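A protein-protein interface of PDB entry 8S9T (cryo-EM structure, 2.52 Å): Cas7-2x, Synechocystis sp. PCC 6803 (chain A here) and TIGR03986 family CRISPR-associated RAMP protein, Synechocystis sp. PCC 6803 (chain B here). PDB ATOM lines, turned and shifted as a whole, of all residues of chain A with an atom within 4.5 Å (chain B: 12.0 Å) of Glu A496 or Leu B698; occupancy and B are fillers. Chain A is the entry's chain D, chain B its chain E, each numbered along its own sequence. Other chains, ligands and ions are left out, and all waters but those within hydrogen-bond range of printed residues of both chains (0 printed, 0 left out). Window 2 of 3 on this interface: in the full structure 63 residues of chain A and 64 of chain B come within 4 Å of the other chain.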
ATOM      1  N   ARG A 443     -31.088  11.623  -3.473  1.00  0.00           N
ATOM      2  CA  ARG A 443     -30.493  10.464  -2.823  1.00  0.00           C
ATOM      3  C   ARG A 443     -30.196  10.722  -1.348  1.00  0.00           C
ATOM      4  O   ARG A 443     -30.393   9.838  -0.512  1.00  0.00           O
ATOM      5  CB  ARG A 443     -29.242  10.029  -3.584  1.00  0.00           C
ATOM      6  CG  ARG A 443     -28.654   8.721  -3.108  1.00  0.00           C
ATOM      7  CD  ARG A 443     -27.537   8.264  -3.981  1.00  0.00           C
ATOM      8  NE  ARG A 443     -26.343   9.067  -3.786  1.00  0.00           N
ATOM      9  CZ  ARG A 443     -25.264   8.986  -4.548  1.00  0.00           C
ATOM     10  NH1 ARG A 443     -25.232   8.137  -5.552  1.00  0.00           N
ATOM     11  NH2 ARG A 443     -24.229   9.769  -4.327  1.00  0.00           N
ATOM     12  N   LEU A 494     -33.767   4.347 -11.548  1.00  0.00           N
ATOM     13  CA  LEU A 494     -33.307   5.006 -12.758  1.00  0.00           C
ATOM     14  C   LEU A 494     -32.382   4.102 -13.558  1.00  0.00           C
ATOM     15  O   LEU A 494     -31.560   3.379 -12.995  1.00  0.00           O
ATOM     16  CB  LEU A 494     -32.603   6.301 -12.400  1.00  0.00           C
ATOM     17  CG  LEU A 494     -33.515   7.363 -11.806  1.00  0.00           C
ATOM     18  CD1 LEU A 494     -32.683   8.469 -11.192  1.00  0.00           C
ATOM     19  CD2 LEU A 494     -34.455   7.899 -12.852  1.00  0.00           C
ATOM     20  N   ASP A 495     -32.562   4.108 -14.877  1.00  0.00           N
ATOM     21  CA  ASP A 495     -31.784   3.239 -15.748  1.00  0.00           C
ATOM     22  C   ASP A 495     -30.296   3.454 -15.540  1.00  0.00           C
ATOM     23  O   ASP A 495     -29.815   4.588 -15.537  1.00  0.00           O
ATOM     24  CB  ASP A 495     -32.148   3.483 -17.211  1.00  0.00           C
ATOM     25  CG  ASP A 495     -33.620   3.311 -17.474  1.00  0.00           C
ATOM     26  OD1 ASP A 495     -34.354   2.999 -16.517  1.00  0.00           O
ATOM     27  OD2 ASP A 495     -34.048   3.466 -18.633  1.00  0.00           O
ATOM     28  N   GLU A 496     -29.569   2.351 -15.371  1.00  0.00           N
ATOM     29  CA  GLU A 496     -28.148   2.447 -15.077  1.00  0.00           C
ATOM     30  C   GLU A 496     -27.383   3.104 -16.215  1.00  0.00           C
ATOM     31  O   GLU A 496     -26.419   3.835 -15.971  1.00  0.00           O
ATOM     32  CB  GLU A 496     -27.590   1.064 -14.772  1.00  0.00           C
ATOM     33  CG  GLU A 496     -26.193   1.093 -14.219  1.00  0.00           C
ATOM     34  CD  GLU A 496     -25.750  -0.253 -13.704  1.00  0.00           C
ATOM     35  OE1 GLU A 496     -24.530  -0.443 -13.505  1.00  0.00           O
ATOM     36  OE2 GLU A 496     -26.623  -1.120 -13.481  1.00  0.00           O
ATOM     37  N   ALA A 497     -27.798   2.863 -17.457  1.00  0.00           N
ATOM     38  CA  ALA A 497     -27.193   3.553 -18.587  1.00  0.00           C
ATOM     39  C   ALA A 497     -27.454   5.047 -18.520  1.00  0.00           C
ATOM     40  O   ALA A 497     -26.597   5.853 -18.893  1.00  0.00           O
ATOM     41  CB  ALA A 497     -27.722   2.977 -19.896  1.00  0.00           C
ATOM     42  N   PHE A 498     -28.643   5.437 -18.068  1.00  0.00           N
ATOM     43  CA  PHE A 498     -28.938   6.848 -17.853  1.00  0.00           C
ATOM     44  C   PHE A 498     -28.191   7.409 -16.648  1.00  0.00           C
ATOM     45  O   PHE A 498     -27.670   8.525 -16.705  1.00  0.00           O
ATOM     46  CB  PHE A 498     -30.442   7.032 -17.699  1.00  0.00           C
ATOM     47  CG  PHE A 498     -30.847   8.412 -17.324  1.00  0.00           C
ATOM     48  CD1 PHE A 498     -30.654   9.463 -18.191  1.00  0.00           C
ATOM     49  CD2 PHE A 498     -31.451   8.655 -16.107  1.00  0.00           C
ATOM     50  CE1 PHE A 498     -31.039  10.727 -17.848  1.00  0.00           C
ATOM     51  CE2 PHE A 498     -31.833   9.923 -15.763  1.00  0.00           C
ATOM     52  CZ  PHE A 498     -31.627  10.961 -16.636  1.00  0.00           C
ATOM     53  N   ARG A 499     -28.141   6.666 -15.542  1.00  0.00           N
ATOM     54  CA  ARG A 499     -27.362   7.116 -14.394  1.00  0.00           C
ATOM     55  C   ARG A 499     -25.872   7.143 -14.678  1.00  0.00           C
ATOM     56  O   ARG A 499     -25.165   7.997 -14.141  1.00  0.00           O
ATOM     57  CB  ARG A 499     -27.654   6.244 -13.182  1.00  0.00           C
ATOM     58  CG  ARG A 499     -29.004   6.507 -12.607  1.00  0.00           C
ATOM     59  CD  ARG A 499     -29.263   5.699 -11.382  1.00  0.00           C
ATOM     60  NE  ARG A 499     -29.402   4.284 -11.677  1.00  0.00           N
ATOM     61  CZ  ARG A 499     -28.611   3.337 -11.200  1.00  0.00           C
ATOM     62  NH1 ARG A 499     -27.611   3.647 -10.394  1.00  0.00           N
ATOM     63  NH2 ARG A 499     -28.828   2.076 -11.521  1.00  0.00           N
ATOM     64  N   GLN A 500     -25.368   6.224 -15.491  1.00  0.00           N
ATOM     65  CA  GLN A 500     -23.983   6.322 -15.924  1.00  0.00           C
ATOM     66  C   GLN A 500     -23.800   7.489 -16.878  1.00  0.00           C
ATOM     67  O   GLN A 500     -22.764   8.161 -16.861  1.00  0.00           O
ATOM     68  CB  GLN A 500     -23.530   5.017 -16.561  1.00  0.00           C
ATOM     69  CG  GLN A 500     -22.068   4.994 -16.905  1.00  0.00           C
ATOM     70  CD  GLN A 500     -21.625   3.634 -17.368  1.00  0.00           C
ATOM     71  OE1 GLN A 500     -22.452   2.773 -17.664  1.00  0.00           O
ATOM     72  NE2 GLN A 500     -20.316   3.424 -17.429  1.00  0.00           N
ATOM     73  N   SER A 503     -23.787  10.378 -14.636  1.00  0.00           N
ATOM     74  CA  SER A 503     -22.525  10.299 -13.906  1.00  0.00           C
ATOM     75  C   SER A 503     -21.328  10.738 -14.733  1.00  0.00           C
ATOM     76  O   SER A 503     -20.353  11.235 -14.173  1.00  0.00           O
ATOM     77  CB  SER A 503     -22.308   8.884 -13.395  1.00  0.00           C
ATOM     78  OG  SER A 503     -23.357   8.517 -12.533  1.00  0.00           O
ATOM     79  N   ASP B 683     -21.701   3.934   8.423  1.00  0.00           N
ATOM     80  CA  ASP B 683     -21.024   4.388   7.201  1.00  0.00           C
ATOM     81  C   ASP B 683     -20.330   5.715   7.510  1.00  0.00           C
ATOM     82  O   ASP B 683     -20.934   6.779   7.408  1.00  0.00           O
ATOM     83  CB  ASP B 683     -22.007   4.527   6.049  1.00  0.00           C
ATOM     84  CG  ASP B 683     -21.350   4.972   4.750  1.00  0.00           C
ATOM     85  OD1 ASP B 683     -20.116   5.146   4.701  1.00  0.00           O
ATOM     86  OD2 ASP B 683     -22.075   5.150   3.755  1.00  0.00           O
ATOM     87  N   ARG B 685     -17.012   8.165   6.489  1.00  0.00           N
ATOM     88  CA  ARG B 685     -15.969   8.476   5.522  1.00  0.00           C
ATOM     89  C   ARG B 685     -15.407   9.855   5.812  1.00  0.00           C
ATOM     90  O   ARG B 685     -16.073  10.691   6.414  1.00  0.00           O
ATOM     91  CB  ARG B 685     -16.463   8.453   4.078  1.00  0.00           C
ATOM     92  CG  ARG B 685     -17.464   7.410   3.780  1.00  0.00           C
ATOM     93  CD  ARG B 685     -17.871   7.472   2.366  1.00  0.00           C
ATOM     94  NE  ARG B 685     -19.010   6.609   2.125  1.00  0.00           N
ATOM     95  CZ  ARG B 685     -19.305   6.080   0.954  1.00  0.00           C
ATOM     96  NH1 ARG B 685     -18.456   6.193  -0.046  1.00  0.00           N
ATOM     97  NH2 ARG B 685     -20.374   5.322   0.831  1.00  0.00           N
ATOM     98  N   GLY B 689     -13.494  10.589   0.870  1.00  0.00           N
ATOM     99  CA  GLY B 689     -14.429   9.516   0.585  1.00  0.00           C
ATOM    100  C   GLY B 689     -15.820   9.981   0.198  1.00  0.00           C
ATOM    101  O   GLY B 689     -16.491   9.336  -0.606  1.00  0.00           O
ATOM    102  N   TRP B 690     -16.289  11.077   0.788  1.00  0.00           N
ATOM    103  CA  TRP B 690     -17.564  11.645   0.365  1.00  0.00           C
ATOM    104  C   TRP B 690     -17.462  12.308  -0.995  1.00  0.00           C
ATOM    105  O   TRP B 690     -18.417  12.290  -1.768  1.00  0.00           O
ATOM    106  CB  TRP B 690     -18.093  12.631   1.406  1.00  0.00           C
ATOM    107  CG  TRP B 690     -18.550  11.949   2.633  1.00  0.00           C
ATOM    108  CD1 TRP B 690     -18.026  12.074   3.869  1.00  0.00           C
ATOM    109  CD2 TRP B 690     -19.584  10.970   2.732  1.00  0.00           C
ATOM    110  NE1 TRP B 690     -18.683  11.266   4.745  1.00  0.00           N
ATOM    111  CE2 TRP B 690     -19.644  10.569   4.072  1.00  0.00           C
ATOM    112  CE3 TRP B 690     -20.474  10.401   1.816  1.00  0.00           C
ATOM    113  CZ2 TRP B 690     -20.550   9.621   4.526  1.00  0.00           C
ATOM    114  CZ3 TRP B 690     -21.376   9.464   2.271  1.00  0.00           C
ATOM    115  CH2 TRP B 690     -21.409   9.087   3.613  1.00  0.00           C
ATOM    116  N   ARG B 691     -16.326  12.922  -1.287  1.00  0.00           N
ATOM    117  CA  ARG B 691     -16.092  13.491  -2.604  1.00  0.00           C
ATOM    118  C   ARG B 691     -16.172  12.426  -3.696  1.00  0.00           C
ATOM    119  O   ARG B 691     -16.645  12.697  -4.802  1.00  0.00           O
ATOM    120  CB  ARG B 691     -14.759  14.239  -2.571  1.00  0.00           C
ATOM    121  CG  ARG B 691     -14.317  14.919  -3.821  1.00  0.00           C
ATOM    122  CD  ARG B 691     -13.153  14.211  -4.442  1.00  0.00           C
ATOM    123  NE  ARG B 691     -11.933  14.435  -3.671  1.00  0.00           N
ATOM    124  CZ  ARG B 691     -11.051  13.490  -3.366  1.00  0.00           C
ATOM    125  NH1 ARG B 691     -11.292  12.224  -3.676  1.00  0.00           N
ATOM    126  NH2 ARG B 691      -9.964  13.802  -2.678  1.00  0.00           N
ATOM    127  N   ASP B 692     -15.716  11.209  -3.406  1.00  0.00           N
ATOM    128  CA  ASP B 692     -15.900  10.094  -4.333  1.00  0.00           C
ATOM    129  C   ASP B 692     -17.349   9.622  -4.385  1.00  0.00           C
ATOM    130  O   ASP B 692     -17.828   9.192  -5.437  1.00  0.00           O
ATOM    131  CB  ASP B 692     -14.998   8.932  -3.941  1.00  0.00           C
ATOM    132  CG  ASP B 692     -13.543   9.308  -3.933  1.00  0.00           C
ATOM    133  OD1 ASP B 692     -13.207  10.402  -4.419  1.00  0.00           O
ATOM    134  OD2 ASP B 692     -12.723   8.517  -3.431  1.00  0.00           O
ATOM    135  N   TYR B 693     -18.043   9.648  -3.252  1.00  0.00           N
ATOM    136  CA  TYR B 693     -19.445   9.251  -3.205  1.00  0.00           C
ATOM    137  C   TYR B 693     -20.345  10.178  -4.014  1.00  0.00           C
ATOM    138  O   TYR B 693     -21.214   9.720  -4.759  1.00  0.00           O
ATOM    139  CB  TYR B 693     -19.886   9.221  -1.751  1.00  0.00           C
ATOM    140  CG  TYR B 693     -21.337   8.947  -1.522  1.00  0.00           C
ATOM    141  CD1 TYR B 693     -21.821   7.660  -1.503  1.00  0.00           C
ATOM    142  CD2 TYR B 693     -22.223   9.979  -1.301  1.00  0.00           C
ATOM    143  CE1 TYR B 693     -23.135   7.415  -1.278  1.00  0.00           C
ATOM    144  CE2 TYR B 693     -23.532   9.739  -1.081  1.00  0.00           C
ATOM    145  CZ  TYR B 693     -23.985   8.456  -1.071  1.00  0.00           C
ATOM    146  OH  TYR B 693     -25.308   8.210  -0.845  1.00  0.00           O
ATOM    147  N   TYR B 694     -20.173  11.483  -3.862  1.00  0.00           N
ATOM    148  CA  TYR B 694     -20.925  12.438  -4.658  1.00  0.00           C
ATOM    149  C   TYR B 694     -20.410  12.572  -6.073  1.00  0.00           C
ATOM    150  O   TYR B 694     -21.070  13.207  -6.895  1.00  0.00           O
ATOM    151  CB  TYR B 694     -20.949  13.795  -3.964  1.00  0.00           C
ATOM    152  CG  TYR B 694     -21.685  13.730  -2.660  1.00  0.00           C
ATOM    153  CD1 TYR B 694     -22.993  13.306  -2.623  1.00  0.00           C
ATOM    154  CD2 TYR B 694     -21.075  14.074  -1.467  1.00  0.00           C
ATOM    155  CE1 TYR B 694     -23.673  13.232  -1.452  1.00  0.00           C
ATOM    156  CE2 TYR B 694     -21.750  14.001  -0.286  1.00  0.00           C
ATOM    157  CZ  TYR B 694     -23.055  13.583  -0.284  1.00  0.00           C
ATOM    158  OH  TYR B 694     -23.766  13.480   0.879  1.00  0.00           O
ATOM    159  N   GLY B 695     -19.247  12.027  -6.364  1.00  0.00           N
ATOM    160  CA  GLY B 695     -18.762  11.967  -7.713  1.00  0.00           C
ATOM    161  C   GLY B 695     -19.486  11.015  -8.631  1.00  0.00           C
ATOM    162  O   GLY B 695     -19.129  10.956  -9.808  1.00  0.00           O
ATOM    163  N   SER B 696     -20.501  10.296  -8.166  1.00  0.00           N
ATOM    164  CA  SER B 696     -21.167   9.331  -9.023  1.00  0.00           C
ATOM    165  C   SER B 696     -22.621   9.165  -8.618  1.00  0.00           C
ATOM    166  O   SER B 696     -22.961   9.217  -7.438  1.00  0.00           O
ATOM    167  CB  SER B 696     -20.458   7.981  -8.964  1.00  0.00           C
ATOM    168  OG  SER B 696     -20.884   7.126 -10.003  1.00  0.00           O
ATOM    169  N   LEU B 697     -23.471   8.927  -9.613  1.00  0.00           N
ATOM    170  CA  LEU B 697     -24.835   8.476  -9.385  1.00  0.00           C
ATOM    171  C   LEU B 697     -24.954   6.963  -9.335  1.00  0.00           C
ATOM    172  O   LEU B 697     -26.012   6.450  -8.961  1.00  0.00           O
ATOM    173  CB  LEU B 697     -25.766   9.026 -10.466  1.00  0.00           C
ATOM    174  CG  LEU B 697     -26.231  10.480 -10.371  1.00  0.00           C
ATOM    175  CD1 LEU B 697     -25.100  11.443 -10.640  1.00  0.00           C
ATOM    176  CD2 LEU B 697     -27.312  10.699 -11.381  1.00  0.00           C
ATOM    177  N   LEU B 698     -23.905   6.246  -9.706  1.00  0.00           N
ATOM    178  CA  LEU B 698     -23.860   4.804  -9.570  1.00  0.00           C
ATOM    179  C   LEU B 698     -23.401   4.407  -8.176  1.00  0.00           C
ATOM    180  O   LEU B 698     -22.628   5.115  -7.529  1.00  0.00           O
ATOM    181  CB  LEU B 698     -22.928   4.200 -10.615  1.00  0.00           C
ATOM    182  CG  LEU B 698     -23.232   4.537 -12.069  1.00  0.00           C
ATOM    183  CD1 LEU B 698     -22.197   3.895 -12.949  1.00  0.00           C
ATOM    184  CD2 LEU B 698     -24.603   4.056 -12.433  1.00  0.00           C
ATOM    185  N   GLU B 699     -23.895   3.262  -7.720  1.00  0.00           N
ATOM    186  CA  GLU B 699     -23.438   2.656  -6.478  1.00  0.00           C
ATOM    187  C   GLU B 699     -21.928   2.473  -6.484  1.00  0.00           C
ATOM    188  O   GLU B 699     -21.337   2.071  -7.487  1.00  0.00           O
ATOM    189  CB  GLU B 699     -24.111   1.296  -6.271  1.00  0.00           C
ATOM    190  CG  GLU B 699     -25.564   1.213  -6.728  1.00  0.00           C
ATOM    191  CD  GLU B 699     -25.697   0.985  -8.233  1.00  0.00           C
ATOM    192  OE1 GLU B 699     -25.452  -0.148  -8.693  1.00  0.00           O
ATOM    193  OE2 GLU B 699     -26.045   1.943  -8.956  1.00  0.00           O
ATOM    194  N   THR B 700     -21.306   2.754  -5.346  1.00  0.00           N
ATOM    195  CA  THR B 700     -19.863   2.855  -5.240  1.00  0.00           C
ATOM    196  C   THR B 700     -19.449   2.197  -3.930  1.00  0.00           C
ATOM    197  O   THR B 700     -20.257   2.068  -3.009  1.00  0.00           O
ATOM    198  CB  THR B 700     -19.418   4.321  -5.314  1.00  0.00           C
ATOM    199  OG1 THR B 700     -19.744   4.846  -6.606  1.00  0.00           O
ATOM    200  CG2 THR B 700     -17.927   4.460  -5.118  1.00  0.00           C
ATOM    201  N   SER B 701     -18.205   1.730  -3.870  1.00  0.00           N
ATOM    202  CA  SER B 701     -17.705   1.106  -2.655  1.00  0.00           C
ATOM    203  C   SER B 701     -17.721   2.081  -1.487  1.00  0.00           C
ATOM    204  O   SER B 701     -17.357   3.248  -1.624  1.00  0.00           O
ATOM    205  CB  SER B 701     -16.285   0.592  -2.871  1.00  0.00           C
ATOM    206  OG  SER B 701     -15.421   1.648  -3.233  1.00  0.00           O
ATOM    207  N   GLN B 702     -18.153   1.594  -0.332  1.00  0.00           N
ATOM    208  CA  GLN B 702     -17.916   2.376   0.868  1.00  0.00           C
ATOM    209  C   GLN B 702     -16.703   1.846   1.619  1.00  0.00           C
ATOM    210  O   GLN B 702     -16.524   0.632   1.733  1.00  0.00           O
ATOM    211  CB  GLN B 702     -19.136   2.368   1.788  1.00  0.00           C
ATOM    212  CG  GLN B 702     -19.539   1.027   2.352  1.00  0.00           C
ATOM    213  CD  GLN B 702     -20.685   1.151   3.338  1.00  0.00           C
ATOM    214  OE1 GLN B 702     -20.488   1.537   4.484  1.00  0.00           O
ATOM    215  NE2 GLN B 702     -21.886   0.831   2.892  1.00  0.00           N
ATOM    216  N   PRO B 703     -15.841   2.731   2.114  1.00  0.00           N
ATOM    217  CA  PRO B 703     -14.704   2.273   2.917  1.00  0.00           C
ATOM    218  C   PRO B 703     -15.161   1.631   4.218  1.00  0.00           C
ATOM    219  O   PRO B 703     -16.102   2.090   4.864  1.00  0.00           O
ATOM    220  CB  PRO B 703     -13.917   3.560   3.162  1.00  0.00           C
ATOM    221  CG  PRO B 703     -14.939   4.628   3.110  1.00  0.00           C
ATOM    222  CD  PRO B 703     -15.924   4.199   2.068  1.00  0.00           C
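The backbone carbonyl oxygen (O) of Tyr B693 is in hydrogen-bond range of the guanidinium group (NH2) of Arg A443, 3.0 Å away. The guanidinium group (NH1) of Arg A443 sits at hydrogen-bond distance from the backbone carbonyl oxygen (O) of Ser B696 (3.1 Å). The side-chain carboxylate of Glu B699 is in salt-bridge range of the guanidinium group of Arg A499 (2.7 Å). The backbone NH (N) of Leu B697 lies within hydrogen-bond range of the side-chain hydroxyl (OG) of Ser A503.
The backbone carbonyl oxygen of Leu A494 lies within hydrogen-bond range of the guanidinium group of Arg A499 (2.7 Å). The side-chain hydroxyl (OG) of Ser A503 is in hydrogen-bond range of the backbone carbonyl oxygen (O) of Arg A499 (2.5 Å). N of Leu B698 is in hydrogen-bond range of OG of Ser B696 (3.2 Å). O of Leu B698 lies within hydrogen-bond range of OG1 of Thr B700 (3.0 Å).
Arg A443 touches Leu B697. Leu B698 touches Glu A496. Arg A499 touches Leu B697 (NH1 to O, 3.5 Å). Leu B698 touches Arg A499. Leu B698 touches Gln A500 (CD2 to N, 3.8 Å). Ser B696 touches Ser A503. Ser A503 touches Leu B698 (OG to N, 3.7 Å).
Printed residues of chain B within 4 Å of Arg A443: Tyr B693, Ser B696 and Leu B697. No residue of chain B comes within 4 Å of Asp A495. Of chain B, only Leu B698 comes within 4 Å of Glu A496. Ala A497 touches none of the printed residues of chain B. Arg A499 touches just these residues of chain B: Leu B697, Leu B698 and Glu B699. Of chain B, only Leu B698 comes within 4 Å of Gln A500. Ser A503 touches three residues of chain B. Asp B683 touches none of the printed residues of chain A. Tyr B694 touches none of the printed residues of chain A. Printed residues of chain A within 4 Å of Ser B696: Arg A443 and Ser A503. Of the printed residues of chain A, Leu B697 touches Arg A443, Arg A499 and Ser A503. Leu B698 touches just these residues of chain A: Glu A496, Arg A499, Gln A500 and Ser A503. The nearest printed residue of chain A that does not touch Leu B698 is Arg A443 (4.5 Å). The nearest printed residue of chain A that does not touch Leu B697 is Phe A498 (5.8 Å).
Printed residues of chain B that touch a printed residue of chain A: Tyr B693, Ser B696, Leu B697, Leu B698 and Glu B699. Hydrophobic or aromatic side chains of chain B within 4 Å of the printed part of chain A: Tyr B693, Leu B697 and Leu B698. Along chain B the printed residues that touch a printed residue of chain A span positions 693 to 699. Of the 9 printed residues of chain A, 5 touch a printed residue of chain B. Among the printed residues, Asp or Glu carboxylates within 4 Å of a Lys or Arg side-chain nitrogen of the other chain: Arg A499 with Glu B699 (2.7 Å).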
